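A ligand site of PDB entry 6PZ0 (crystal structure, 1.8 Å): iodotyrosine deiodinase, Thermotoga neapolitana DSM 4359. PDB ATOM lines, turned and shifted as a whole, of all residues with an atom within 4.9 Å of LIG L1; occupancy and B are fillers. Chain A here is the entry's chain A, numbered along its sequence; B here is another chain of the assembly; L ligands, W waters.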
ATOM      1  N   ARG A  11       7.808  26.756 -14.204  1.00  0.00           N
ATOM      2  CA  ARG A  11       7.487  26.058 -12.986  1.00  0.00           C
ATOM      3  C   ARG A  11       6.738  24.794 -13.271  1.00  0.00           C
ATOM      4  O   ARG A  11       5.786  24.780 -14.056  1.00  0.00           O
ATOM      5  CB  ARG A  11       6.662  26.958 -12.078  1.00  0.00           C
ATOM      6  CG  ARG A  11       6.467  26.384 -10.713  1.00  0.00           C
ATOM      7  CD  ARG A  11       5.147  25.736 -10.541  1.00  0.00           C
ATOM      8  NE  ARG A  11       5.169  24.905  -9.350  1.00  0.00           N
ATOM      9  CZ  ARG A  11       4.498  23.759  -9.237  1.00  0.00           C
ATOM     10  NH1 ARG A  11       3.699  23.343 -10.201  1.00  0.00           N
ATOM     11  NH2 ARG A  11       4.613  23.043  -8.133  1.00  0.00           N
ATOM     12  N   LYS A  12       7.193  23.723 -12.626  1.00  0.00           N
ATOM     13  CA  LYS A  12       6.656  22.398 -12.831  1.00  0.00           C
ATOM     14  C   LYS A  12       6.680  21.660 -11.510  1.00  0.00           C
ATOM     15  O   LYS A  12       7.289  22.114 -10.550  1.00  0.00           O
ATOM     16  CB  LYS A  12       7.462  21.640 -13.864  1.00  0.00           C
ATOM     17  CG  LYS A  12       8.889  21.295 -13.450  1.00  0.00           C
ATOM     18  CD  LYS A  12       9.643  20.588 -14.600  1.00  0.00           C
ATOM     19  CE  LYS A  12      11.102  20.290 -14.262  1.00  0.00           C
ATOM     20  NZ  LYS A  12      12.004  21.467 -14.386  1.00  0.00           N
ATOM     21  N   THR A  13       6.019  20.516 -11.488  1.00  0.00           N
ATOM     22  CA  THR A  13       6.008  19.693 -10.283  1.00  0.00           C
ATOM     23  C   THR A  13       7.394  19.276  -9.906  1.00  0.00           C
ATOM     24  O   THR A  13       8.193  18.915 -10.764  1.00  0.00           O
ATOM     25  CB  THR A  13       5.165  18.427 -10.473  1.00  0.00           C
ATOM     26  OG1 THR A  13       3.963  18.733 -11.181  1.00  0.00           O
ATOM     27  CG2 THR A  13       4.809  17.821  -9.140  1.00  0.00           C
ATOM     28  N   ARG A  15       8.837  16.361  -7.371  1.00  0.00           N
ATOM     29  CA  ARG A  15       8.583  15.233  -6.478  1.00  0.00           C
ATOM     30  C   ARG A  15       9.891  14.581  -6.042  1.00  0.00           C
ATOM     31  O   ARG A  15       9.888  13.608  -5.276  1.00  0.00           O
ATOM     32  CB  ARG A  15       7.693  14.189  -7.141  1.00  0.00           C
ATOM     33  CG  ARG A  15       6.327  14.710  -7.513  1.00  0.00           C
ATOM     34  CD  ARG A  15       5.430  13.611  -8.036  1.00  0.00           C
ATOM     35  NE  ARG A  15       4.113  14.080  -8.423  1.00  0.00           N
ATOM     36  CZ  ARG A  15       3.801  14.600  -9.609  1.00  0.00           C
ATOM     37  NH1 ARG A  15       4.711  14.731 -10.555  1.00  0.00           N
ATOM     38  NH2 ARG A  15       2.567  14.991  -9.852  1.00  0.00           N
ATOM     39  N   GLU A  68      -3.480   6.294   0.261  1.00  0.00           N
ATOM     40  CA  GLU A  68      -3.238   6.192  -1.169  1.00  0.00           C
ATOM     41  C   GLU A  68      -3.339   4.756  -1.632  1.00  0.00           C
ATOM     42  O   GLU A  68      -3.904   4.463  -2.671  1.00  0.00           O
ATOM     43  CB  GLU A  68      -1.857   6.732  -1.532  1.00  0.00           C
ATOM     44  CG  GLU A  68      -1.697   8.241  -1.347  1.00  0.00           C
ATOM     45  CD  GLU A  68      -2.497   9.074  -2.322  1.00  0.00           C
ATOM     46  OE1 GLU A  68      -3.359   8.527  -3.063  1.00  0.00           O
ATOM     47  OE2 GLU A  68      -2.245  10.307  -2.313  1.00  0.00           O
ATOM     48  N   TRP A  82      -4.958   8.097 -16.153  1.00  0.00           N
ATOM     49  CA  TRP A  82      -3.864   9.065 -16.126  1.00  0.00           C
ATOM     50  C   TRP A  82      -2.754   8.607 -15.167  1.00  0.00           C
ATOM     51  O   TRP A  82      -1.565   8.641 -15.505  1.00  0.00           O
ATOM     52  CB  TRP A  82      -4.407  10.446 -15.711  1.00  0.00           C
ATOM     53  CG  TRP A  82      -3.414  11.590 -15.795  1.00  0.00           C
ATOM     54  CD1 TRP A  82      -3.125  12.350 -16.884  1.00  0.00           C
ATOM     55  CD2 TRP A  82      -2.587  12.080 -14.732  1.00  0.00           C
ATOM     56  NE1 TRP A  82      -2.178  13.282 -16.580  1.00  0.00           N
ATOM     57  CE2 TRP A  82      -1.832  13.146 -15.269  1.00  0.00           C
ATOM     58  CE3 TRP A  82      -2.423  11.742 -13.390  1.00  0.00           C
ATOM     59  CZ2 TRP A  82      -0.934  13.866 -14.513  1.00  0.00           C
ATOM     60  CZ3 TRP A  82      -1.527  12.455 -12.628  1.00  0.00           C
ATOM     61  CH2 TRP A  82      -0.787  13.518 -13.190  1.00  0.00           C
ATOM     62  N   PHE A  88       2.316   6.392 -11.664  1.00  0.00           N
ATOM     63  CA  PHE A  88       2.150   6.774 -10.253  1.00  0.00           C
ATOM     64  C   PHE A  88       1.877   5.545  -9.409  1.00  0.00           C
ATOM     65  O   PHE A  88       1.231   4.590  -9.879  1.00  0.00           O
ATOM     66  CB  PHE A  88       0.983   7.754 -10.093  1.00  0.00           C
ATOM     67  CG  PHE A  88       1.308   9.182 -10.466  1.00  0.00           C
ATOM     68  CD1 PHE A  88       1.482   9.567 -11.778  1.00  0.00           C
ATOM     69  CD2 PHE A  88       1.418  10.131  -9.479  1.00  0.00           C
ATOM     70  CE1 PHE A  88       1.775  10.880 -12.110  1.00  0.00           C
ATOM     71  CE2 PHE A  88       1.698  11.444  -9.799  1.00  0.00           C
ATOM     72  CZ  PHE A  88       1.883  11.821 -11.116  1.00  0.00           C
ATOM     73  N   PHE A  94       8.566  11.408  -1.197  1.00  0.00           N
ATOM     74  CA  PHE A  94       8.912  12.800  -1.074  1.00  0.00           C
ATOM     75  C   PHE A  94       8.398  13.385   0.237  1.00  0.00           C
ATOM     76  O   PHE A  94       8.888  14.429   0.664  1.00  0.00           O
ATOM     77  CB  PHE A  94       8.383  13.651  -2.240  1.00  0.00           C
ATOM     78  CG  PHE A  94       6.918  13.434  -2.562  1.00  0.00           C
ATOM     79  CD1 PHE A  94       5.927  14.052  -1.830  1.00  0.00           C
ATOM     80  CD2 PHE A  94       6.553  12.642  -3.624  1.00  0.00           C
ATOM     81  CE1 PHE A  94       4.594  13.865  -2.133  1.00  0.00           C
ATOM     82  CE2 PHE A  94       5.214  12.437  -3.952  1.00  0.00           C
ATOM     83  CZ  PHE A  94       4.231  13.060  -3.210  1.00  0.00           C
ATOM     84  N   TRP A 118      -6.759  28.508  -2.086  1.00  0.00           N
ATOM     85  CA  TRP A 118      -6.152  27.941  -3.294  1.00  0.00           C
ATOM     86  C   TRP A 118      -5.597  29.034  -4.224  1.00  0.00           C
ATOM     87  O   TRP A 118      -4.563  28.851  -4.847  1.00  0.00           O
ATOM     88  CB  TRP A 118      -7.143  27.038  -3.999  1.00  0.00           C
ATOM     89  CG  TRP A 118      -7.097  25.731  -3.284  1.00  0.00           C
ATOM     90  CD1 TRP A 118      -7.907  25.315  -2.279  1.00  0.00           C
ATOM     91  CD2 TRP A 118      -6.104  24.717  -3.465  1.00  0.00           C
ATOM     92  NE1 TRP A 118      -7.497  24.062  -1.841  1.00  0.00           N
ATOM     93  CE2 TRP A 118      -6.393  23.682  -2.551  1.00  0.00           C
ATOM     94  CE3 TRP A 118      -5.000  24.585  -4.293  1.00  0.00           C
ATOM     95  CZ2 TRP A 118      -5.627  22.520  -2.475  1.00  0.00           C
ATOM     96  CZ3 TRP A 118      -4.241  23.431  -4.226  1.00  0.00           C
ATOM     97  CH2 TRP A 118      -4.558  22.413  -3.317  1.00  0.00           C
ATOM     98  N   VAL A 136       5.007  20.313  -4.767  1.00  0.00           N
ATOM     99  CA  VAL A 136       3.912  19.605  -5.414  1.00  0.00           C
ATOM    100  C   VAL A 136       2.709  19.753  -4.505  1.00  0.00           C
ATOM    101  O   VAL A 136       2.830  19.589  -3.305  1.00  0.00           O
ATOM    102  CB  VAL A 136       4.207  18.091  -5.706  1.00  0.00           C
ATOM    103  CG1 VAL A 136       4.707  17.379  -4.478  1.00  0.00           C
ATOM    104  CG2 VAL A 136       2.962  17.418  -6.217  1.00  0.00           C
ATOM    105  N   PRO A 137       1.544  20.147  -5.059  1.00  0.00           N
ATOM    106  CA  PRO A 137       0.358  20.207  -4.219  1.00  0.00           C
ATOM    107  C   PRO A 137      -0.114  18.809  -3.957  1.00  0.00           C
ATOM    108  O   PRO A 137      -0.745  18.189  -4.804  1.00  0.00           O
ATOM    109  CB  PRO A 137      -0.650  20.974  -5.072  1.00  0.00           C
ATOM    110  CG  PRO A 137       0.157  21.651  -6.129  1.00  0.00           C
ATOM    111  CD  PRO A 137       1.311  20.745  -6.382  1.00  0.00           C
ATOM    112  N   TYR A 138       0.269  18.287  -2.813  1.00  0.00           N
ATOM    113  CA  TYR A 138      -0.041  16.895  -2.535  1.00  0.00           C
ATOM    114  C   TYR A 138      -1.340  16.808  -1.768  1.00  0.00           C
ATOM    115  O   TYR A 138      -1.500  17.402  -0.710  1.00  0.00           O
ATOM    116  CB  TYR A 138       1.101  16.226  -1.775  1.00  0.00           C
ATOM    117  CG  TYR A 138       0.681  14.836  -1.420  1.00  0.00           C
ATOM    118  CD1 TYR A 138       0.389  13.910  -2.411  1.00  0.00           C
ATOM    119  CD2 TYR A 138       0.507  14.472  -0.099  1.00  0.00           C
ATOM    120  CE1 TYR A 138      -0.044  12.637  -2.079  1.00  0.00           C
ATOM    121  CE2 TYR A 138       0.076  13.227   0.236  1.00  0.00           C
ATOM    122  CZ  TYR A 138      -0.193  12.300  -0.764  1.00  0.00           C
ATOM    123  OH  TYR A 138      -0.653  11.059  -0.436  1.00  0.00           O
ATOM    124  N   THR A 139      -2.272  16.020  -2.312  1.00  0.00           N
ATOM    125  CA  THR A 139      -3.601  15.905  -1.750  1.00  0.00           C
ATOM    126  C   THR A 139      -3.946  14.428  -1.589  1.00  0.00           C
ATOM    127  O   THR A 139      -4.414  13.810  -2.523  1.00  0.00           O
ATOM    128  CB  THR A 139      -4.648  16.587  -2.655  1.00  0.00           C
ATOM    129  OG1 THR A 139      -4.597  16.006  -3.962  1.00  0.00           O
ATOM    130  CG2 THR A 139      -4.369  18.081  -2.786  1.00  0.00           C
ATOM    131  N   PRO A 140      -3.700  13.856  -0.407  1.00  0.00           N
ATOM    132  CA  PRO A 140      -4.072  12.454  -0.181  1.00  0.00           C
ATOM    133  C   PRO A 140      -5.581  12.284  -0.138  1.00  0.00           C
ATOM    134  O   PRO A 140      -6.294  13.262   0.017  1.00  0.00           O
ATOM    135  CB  PRO A 140      -3.458  12.140   1.185  1.00  0.00           C
ATOM    136  CG  PRO A 140      -3.449  13.476   1.882  1.00  0.00           C
ATOM    137  CD  PRO A 140      -3.199  14.501   0.812  1.00  0.00           C
ATOM    138  N   PRO A 172      10.332  16.262 -16.443  1.00  0.00           N
ATOM    139  CA  PRO A 172       9.843  17.393 -17.236  1.00  0.00           C
ATOM    140  C   PRO A 172       8.374  17.739 -17.034  1.00  0.00           C
ATOM    141  O   PRO A 172       7.514  16.902 -16.707  1.00  0.00           O
ATOM    142  CB  PRO A 172      10.048  16.925 -18.674  1.00  0.00           C
ATOM    143  CG  PRO A 172      11.107  15.878 -18.566  1.00  0.00           C
ATOM    144  CD  PRO A 172      10.857  15.182 -17.289  1.00  0.00           C
ATOM    145  N   LYS A 173       8.106  19.017 -17.263  1.00  0.00           N
ATOM    146  CA  LYS A 173       6.767  19.530 -17.200  1.00  0.00           C
ATOM    147  C   LYS A 173       5.889  18.771 -18.158  1.00  0.00           C
ATOM    148  O   LYS A 173       6.322  18.429 -19.265  1.00  0.00           O
ATOM    149  CB  LYS A 173       6.749  21.011 -17.531  1.00  0.00           C
ATOM    150  CG  LYS A 173       5.481  21.682 -17.105  1.00  0.00           C
ATOM    151  CD  LYS A 173       5.570  23.198 -17.161  1.00  0.00           C
ATOM    152  CE  LYS A 173       4.219  23.760 -16.785  1.00  0.00           C
ATOM    153  NZ  LYS A 173       4.286  25.172 -16.411  1.00  0.00           N
ATOM    154  N   TYR A 174       4.666  18.476 -17.747  1.00  0.00           N
ATOM    155  CA  TYR A 174       3.695  17.892 -18.669  1.00  0.00           C
ATOM    156  C   TYR A 174       3.189  18.930 -19.662  1.00  0.00           C
ATOM    157  O   TYR A 174       3.336  20.147 -19.467  1.00  0.00           O
ATOM    158  CB  TYR A 174       2.511  17.298 -17.916  1.00  0.00           C
ATOM    159  CG  TYR A 174       2.884  16.162 -16.975  1.00  0.00           C
ATOM    160  CD1 TYR A 174       4.069  15.457 -17.132  1.00  0.00           C
ATOM    161  CD2 TYR A 174       2.034  15.784 -15.955  1.00  0.00           C
ATOM    162  CE1 TYR A 174       4.401  14.440 -16.271  1.00  0.00           C
ATOM    163  CE2 TYR A 174       2.364  14.779 -15.079  1.00  0.00           C
ATOM    164  CZ  TYR A 174       3.537  14.093 -15.266  1.00  0.00           C
ATOM    165  OH  TYR A 174       3.869  13.075 -14.405  1.00  0.00           O
ATOM    166  N   ARG A 176       0.722  21.361 -21.981  1.00  0.00           N
ATOM    167  CA  ARG A 176      -0.460  22.157 -21.744  1.00  0.00           C
ATOM    168  C   ARG A 176      -1.231  22.312 -23.035  1.00  0.00           C
ATOM    169  O   ARG A 176      -0.697  22.751 -24.042  1.00  0.00           O
ATOM    170  CB  ARG A 176      -0.113  23.544 -21.207  1.00  0.00           C
ATOM    171  CG  ARG A 176       0.507  23.613 -19.824  1.00  0.00           C
ATOM    172  CD  ARG A 176      -0.496  23.162 -18.800  1.00  0.00           C
ATOM    173  NE  ARG A 176      -0.039  23.338 -17.424  1.00  0.00           N
ATOM    174  CZ  ARG A 176       0.824  22.549 -16.809  1.00  0.00           C
ATOM    175  NH1 ARG A 176       1.367  21.510 -17.437  1.00  0.00           N
ATOM    176  NH2 ARG A 176       1.171  22.789 -15.555  1.00  0.00           N
ATOM    177  N   GLU B  36      -0.626  27.889 -17.533  1.00  0.00           N
ATOM    178  CA  GLU B  36       0.600  27.208 -17.162  1.00  0.00           C
ATOM    179  C   GLU B  36       0.572  26.645 -15.758  1.00  0.00           C
ATOM    180  O   GLU B  36       1.483  25.932 -15.374  1.00  0.00           O
ATOM    181  CB  GLU B  36       1.793  28.159 -17.266  1.00  0.00           C
ATOM    182  CG  GLU B  36       2.148  28.469 -18.688  1.00  0.00           C
ATOM    183  CD  GLU B  36       2.552  27.250 -19.471  1.00  0.00           C
ATOM    184  OE1 GLU B  36       3.242  26.353 -18.919  1.00  0.00           O
ATOM    185  OE2 GLU B  36       2.168  27.192 -20.661  1.00  0.00           O
ATOM    186  N   PRO B  38      -0.330  24.474 -12.404  1.00  0.00           N
ATOM    187  CA  PRO B  38      -0.584  23.047 -12.167  1.00  0.00           C
ATOM    188  C   PRO B  38      -2.058  22.804 -11.991  1.00  0.00           C
ATOM    189  O   PRO B  38      -2.817  23.741 -11.740  1.00  0.00           O
ATOM    190  CB  PRO B  38       0.159  22.770 -10.856  1.00  0.00           C
ATOM    191  CG  PRO B  38       0.132  24.086 -10.147  1.00  0.00           C
ATOM    192  CD  PRO B  38       0.348  25.103 -11.254  1.00  0.00           C
ATOM    193  N   SER B  39      -2.473  21.552 -12.111  1.00  0.00           N
ATOM    194  CA  SER B  39      -3.862  21.182 -11.867  1.00  0.00           C
ATOM    195  C   SER B  39      -3.876  19.686 -11.581  1.00  0.00           C
ATOM    196  O   SER B  39      -2.933  18.980 -11.953  1.00  0.00           O
ATOM    197  CB  SER B  39      -4.758  21.496 -13.072  1.00  0.00           C
ATOM    198  OG  SER B  39      -4.354  20.777 -14.230  1.00  0.00           O
ATOM    199  N   GLY B  40      -4.918  19.236 -10.894  1.00  0.00           N
ATOM    200  CA  GLY B  40      -5.077  17.833 -10.561  1.00  0.00           C
ATOM    201  C   GLY B  40      -5.079  17.035 -11.875  1.00  0.00           C
ATOM    202  O   GLY B  40      -5.783  17.379 -12.816  1.00  0.00           O
ATOM    203  N   MET B  41      -4.319  15.945 -11.875  1.00  0.00           N
ATOM    204  CA  MET B  41      -4.062  15.120 -13.068  1.00  0.00           C
ATOM    205  C   MET B  41      -3.828  15.912 -14.363  1.00  0.00           C
ATOM    206  O   MET B  41      -4.096  15.404 -15.497  1.00  0.00           O
ATOM    207  CB  MET B  41      -5.177  14.085 -13.265  1.00  0.00           C
ATOM    208  CG  MET B  41      -6.585  14.597 -13.501  1.00  0.00           C
ATOM    209  SD  MET B  41      -7.624  13.205 -14.124  1.00  0.00           S
ATOM    210  CE  MET B  41      -7.147  13.211 -15.826  1.00  0.00           C
ATOM    211  N   ASN B  42      -3.231  17.089 -14.221  1.00  0.00           N
ATOM    212  CA  ASN B  42      -2.973  17.990 -15.342  1.00  0.00           C
ATOM    213  C   ASN B  42      -4.208  18.160 -16.243  1.00  0.00           C
ATOM    214  O   ASN B  42      -4.112  18.279 -17.470  1.00  0.00           O
ATOM    215  CB  ASN B  42      -1.770  17.528 -16.167  1.00  0.00           C
ATOM    216  CG  ASN B  42      -1.244  18.623 -17.103  1.00  0.00           C
ATOM    217  OD1 ASN B  42      -1.265  19.804 -16.767  1.00  0.00           O
ATOM    218  ND2 ASN B  42      -0.801  18.217 -18.285  1.00  0.00           N
ATOM    219  N   TYR B 112     -10.225  17.457  -8.577  1.00  0.00           N
ATOM    220  CA  TYR B 112      -9.545  18.615  -8.025  1.00  0.00           C
ATOM    221  C   TYR B 112      -9.786  19.871  -8.854  1.00  0.00           C
ATOM    222  O   TYR B 112      -8.935  20.779  -8.872  1.00  0.00           O
ATOM    223  CB  TYR B 112      -8.046  18.360  -7.944  1.00  0.00           C
ATOM    224  CG  TYR B 112      -7.705  16.968  -7.489  1.00  0.00           C
ATOM    225  CD1 TYR B 112      -7.681  16.671  -6.147  1.00  0.00           C
ATOM    226  CD2 TYR B 112      -7.438  15.944  -8.403  1.00  0.00           C
ATOM    227  CE1 TYR B 112      -7.400  15.377  -5.704  1.00  0.00           C
ATOM    228  CE2 TYR B 112      -7.153  14.652  -7.975  1.00  0.00           C
ATOM    229  CZ  TYR B 112      -7.130  14.382  -6.616  1.00  0.00           C
ATOM    230  OH  TYR B 112      -6.858  13.110  -6.167  1.00  0.00           O
ATOM    231  N   GLU B 115     -10.089  23.379  -6.776  1.00  0.00           N
ATOM    232  CA  GLU B 115      -8.800  23.746  -6.236  1.00  0.00           C
ATOM    233  C   GLU B 115      -7.869  24.232  -7.338  1.00  0.00           C
ATOM    234  O   GLU B 115      -7.174  25.244  -7.202  1.00  0.00           O
ATOM    235  CB  GLU B 115      -8.202  22.574  -5.487  1.00  0.00           C
ATOM    236  CG  GLU B 115      -9.035  22.217  -4.257  1.00  0.00           C
ATOM    237  CD  GLU B 115      -8.575  20.964  -3.575  1.00  0.00           C
ATOM    238  OE1 GLU B 115      -7.957  20.092  -4.230  1.00  0.00           O
ATOM    239  OE2 GLU B 115      -8.843  20.839  -2.366  1.00  0.00           O
ATOM    240  N   SER B 116      -7.894  23.524  -8.455  1.00  0.00           N
ATOM    241  CA  SER B 116      -7.012  23.843  -9.552  1.00  0.00           C
ATOM    242  C   SER B 116      -7.370  25.162 -10.199  1.00  0.00           C
ATOM    243  O   SER B 116      -6.506  25.912 -10.583  1.00  0.00           O
ATOM    244  CB  SER B 116      -7.076  22.756 -10.627  1.00  0.00           C
ATOM    245  OG  SER B 116      -6.581  21.526 -10.146  1.00  0.00           O
ATOM    246  N   LEU B 119      -6.360  28.042  -7.931  1.00  0.00           N
ATOM    247  CA  LEU B 119      -4.923  28.184  -7.985  1.00  0.00           C
ATOM    248  C   LEU B 119      -4.575  28.983  -9.232  1.00  0.00           C
ATOM    249  O   LEU B 119      -3.844  29.965  -9.185  1.00  0.00           O
ATOM    250  CB  LEU B 119      -4.266  26.789  -7.989  1.00  0.00           C
ATOM    251  CG  LEU B 119      -2.754  26.752  -7.815  1.00  0.00           C
ATOM    252  CD1 LEU B 119      -2.399  25.386  -7.275  1.00  0.00           C
ATOM    253  CD2 LEU B 119      -1.991  27.034  -9.096  1.00  0.00           C
HETATM  254  N1  LIG L   1       0.538  15.493  -7.634  1.00  0.00           N
HETATM  255  C1  LIG L   1       0.736  14.329  -6.983  1.00  0.00           C
HETATM  256  O1  LIG L   1       1.718  13.664  -7.226  1.00  0.00           O
HETATM  257  N2  LIG L   1      -0.178  13.909  -6.067  1.00  0.00           N
HETATM  258  C2  LIG L   1      -1.291  14.642  -5.754  1.00  0.00           C
HETATM  259  O2  LIG L   1      -2.086  14.220  -4.913  1.00  0.00           O
HETATM  260  C3  LIG L   1      -1.491  15.844  -6.424  1.00  0.00           C
HETATM  261  N3  LIG L   1      -2.603  16.615  -6.144  1.00  0.00           N
HETATM  262  C4  LIG L   1      -2.778  17.820  -6.787  1.00  0.00           C
HETATM  263  C5  LIG L   1      -3.897  18.589  -6.479  1.00  0.00           C
HETATM  264  C6  LIG L   1      -4.103  19.816  -7.106  1.00  0.00           C
HETATM  265  C7  LIG L   1      -5.314  20.622  -6.736  1.00  0.00           C
HETATM  266  C8  LIG L   1      -3.172  20.250  -8.045  1.00  0.00           C
HETATM  267  C9  LIG L   1      -3.384  21.579  -8.694  1.00  0.00           C
HETATM  268  C10 LIG L   1      -2.051  19.482  -8.367  1.00  0.00           C
HETATM  269  C11 LIG L   1      -1.844  18.255  -7.740  1.00  0.00           C
HETATM  270  N4  LIG L   1      -0.730  17.450  -8.045  1.00  0.00           N
HETATM  271  C12 LIG L   1      -0.564  16.263  -7.351  1.00  0.00           C
HETATM  272  C13 LIG L   1       0.288  17.884  -9.051  1.00  0.00           C
HETATM  273  C14 LIG L   1      -0.246  17.642 -10.487  1.00  0.00           C
HETATM  274  O3  LIG L   1      -0.146  16.272 -10.849  1.00  0.00           O
HETATM  275  C15 LIG L   1       0.507  18.518 -11.483  1.00  0.00           C
HETATM  276  O4  LIG L   1       0.192  19.855 -11.187  1.00  0.00           O
HETATM  277  C16 LIG L   1       0.163  18.228 -12.959  1.00  0.00           C
HETATM  278  O5  LIG L   1       0.588  16.925 -13.270  1.00  0.00           O
HETATM  279  C17 LIG L   1       0.864  19.192 -13.865  1.00  0.00           C
HETATM  280  O6  LIG L   1       2.251  19.135 -13.597  1.00  0.00           O
HETATM  281  P1  LIG L   1       3.246  20.030 -14.420  1.00  0.00           P
HETATM  282  O7  LIG L   1       4.667  19.635 -14.004  1.00  0.00           O
HETATM  283  O8  LIG L   1       3.016  21.485 -14.081  1.00  0.00           O
HETATM  284  O9  LIG L   1       2.996  19.840 -15.903  1.00  0.00           O
HETATM  285  N1  LG2 L   2      -3.049  11.653  -4.666  1.00  0.00           N
HETATM  286  C1  LG2 L   2      -2.661  10.521  -5.525  1.00  0.00           C
HETATM  287  C2  LG2 L   2      -1.144  10.444  -5.673  1.00  0.00           C
HETATM  288  O1  LG2 L   2      -0.625   9.505  -6.284  1.00  0.00           O
HETATM  289  C3  LG2 L   2      -3.337  10.626  -6.893  1.00  0.00           C
HETATM  290  C4  LG2 L   2      -3.084  11.900  -7.673  1.00  0.00           C
HETATM  291  C5  LG2 L   2      -1.870  12.111  -8.318  1.00  0.00           C
HETATM  292  C6  LG2 L   2      -4.068  12.864  -7.792  1.00  0.00           C
HETATM  293  C7  LG2 L   2      -1.648  13.270  -9.056  1.00  0.00           C
HETATM  294  C8  LG2 L   2      -3.851  14.019  -8.553  1.00  0.00           C
HETATM  295  C9  LG2 L   2      -2.638  14.211  -9.157  1.00  0.00           C
HETATM  296  O2  LG2 L   2      -2.431  15.363  -9.877  1.00  0.00           O
HETATM  297  O3  LG2 L   2      -0.435  11.336  -5.194  1.00  0.00           O
HETATM  298  O   HOH W   1       3.315  16.501 -12.581  1.00  0.00           O
HETATM  299  O   HOH W   2       2.951  11.460  -6.305  1.00  0.00           O
HETATM  300  O   HOH W   3       5.615  17.233 -14.458  1.00  0.00           O
HETATM  301  O   HOH W   4       3.147  23.888 -12.960  1.00  0.00           O
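Water W3 lies within hydrogen-bond range of an oxygen (O7) of LIG L1 and the backbone carbonyl oxygen of Pro 172. Water W4 lies within hydrogen-bond range of O8 of LIG L1 (2.7 Å), NH1 of Arg 11 (2.9 Å) and NH2 of Arg 176 (3.4 Å). Water W1 lies within hydrogen-bond range of the side-chain hydroxyl (OG1) of Thr 13 (2.7 Å), an oxygen (O5) of LIG L1 (2.8 Å) and the guanidinium group (NH1) of Arg 15 (3.0 Å).
An oxygen (O2) of LG2 L2 sits at hydrogen-bond distance from an oxygen (O3) of LIG L1 (2.6 Å).
The backbone carbonyl oxygen (O) of Thr 139 is in hydrogen-bond range of a nitrogen (N1) of LG2 L2, 3.3 Å away. An oxygen (O4) of LIG L1 sits at hydrogen-bond distance from the backbone carbonyl oxygen of Ser 39 of chain B (3.3 Å). OG1 of Thr 13 is in hydrogen-bond range of O6 of LIG L1. O1 of LIG L1 lies within hydrogen-bond range of NE of Arg 15 (2.7 Å). OG1 of Thr 139 lies within hydrogen-bond range of N3 of LIG L1, 3.0 Å away. An oxygen (O2) of LG2 L2 sits at hydrogen-bond distance from the backbone NH (N) of Met 41 of chain B, 2.8 Å away. The backbone NH of Thr 139 is in hydrogen-bond range of an oxygen (O2) of LIG L1 (3.2 Å). OE2 of Glu 68 is in salt-bridge range of N1 of LG2 L2, 2.8 Å away. O4 of LIG L1 sits at hydrogen-bond distance from N of Ser 39 of chain B (3.3 Å). O9 of LIG L1 is in hydrogen-bond range of N of Tyr 174 (2.8 Å). An oxygen (O8) of LIG L1 lies within salt-bridge range of the guanidinium group of Arg 176 (2.7 Å). N of Thr 13 lies within hydrogen-bond range of O7 of LIG L1 (3.0 Å).
The side-chain carboxylate of Glu 68 is in hydrogen-bond range of the side-chain hydroxyl of Tyr 138, 2.6 Å away. OD1 of Asn 42 of chain B sits at hydrogen-bond distance from NH1 of Arg 176 (3.2 Å). The side-chain amino group of Lys 173 lies within salt-bridge range of the side-chain carboxylate of Glu 36 of chain B. The guanidinium group (NH2) of Arg 176 lies within hydrogen-bond range of the backbone carbonyl oxygen (O) of Glu 36 of chain B (3.2 Å). The indole nitrogen of Trp 82 lies within hydrogen-bond range of the backbone carbonyl oxygen of Met 41 of chain B (3.1 Å). The side-chain amino group (NZ) of Lys 173 lies within hydrogen-bond range of the backbone carbonyl oxygen (O) of Arg 11, 2.8 Å away. OG of Ser 116 of chain B is in hydrogen-bond range of N of Gly 40 of chain B. O of Tyr 174 lies within hydrogen-bond range of NH1 of Arg 176 (3.1 Å).
The backbone carbonyl oxygen of Pro 137 lies close to a nitrogen (N3) of LIG L1 (2.8 Å). Lys 12 touches LIG L1 (CB to O7, 3.4 Å). Trp 82 touches LIG L1. Phe 88 touches LIG L1. Trp 118 touches LIG L1. Val 136 touches LIG L1 (CG2 to N1, 3.4 Å). CD1 of Tyr 138 touches O2 of LIG L1 (3.5 Å). Lys 173 touches LIG L1. CB of Pro 38 of chain B touches O4 of LIG L1 (2.9 Å). Gly 40 of chain B touches LIG L1. OD1 of Asn 42 of chain B touches C17 of LIG L1 (3.7 Å). CB of Tyr 112 of chain B touches C7 of LIG L1 (3.7 Å). OE1 of Glu 115 of chain B touches C7 of LIG L1 (3.7 Å). Ser 116 of chain B touches LIG L1. 20 residues have an atom within 4 Å of LIG L1: Lys 12, Thr 13, Arg 15, Trp 82, Phe 88, Trp 118, Val 136, Pro 137, Tyr 138, Thr 139, Lys 173, Tyr 174, Arg 176, Pro 38 of chain B, Ser 39 of chain B, Gly 40 of chain B, Asn 42 of chain B, Tyr 112 of chain B, Glu 115 of chain B and Ser 116 of chain B. The nearest printed residue that does not touch LIG L1 is Leu 119 of chain B (4.2 Å).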
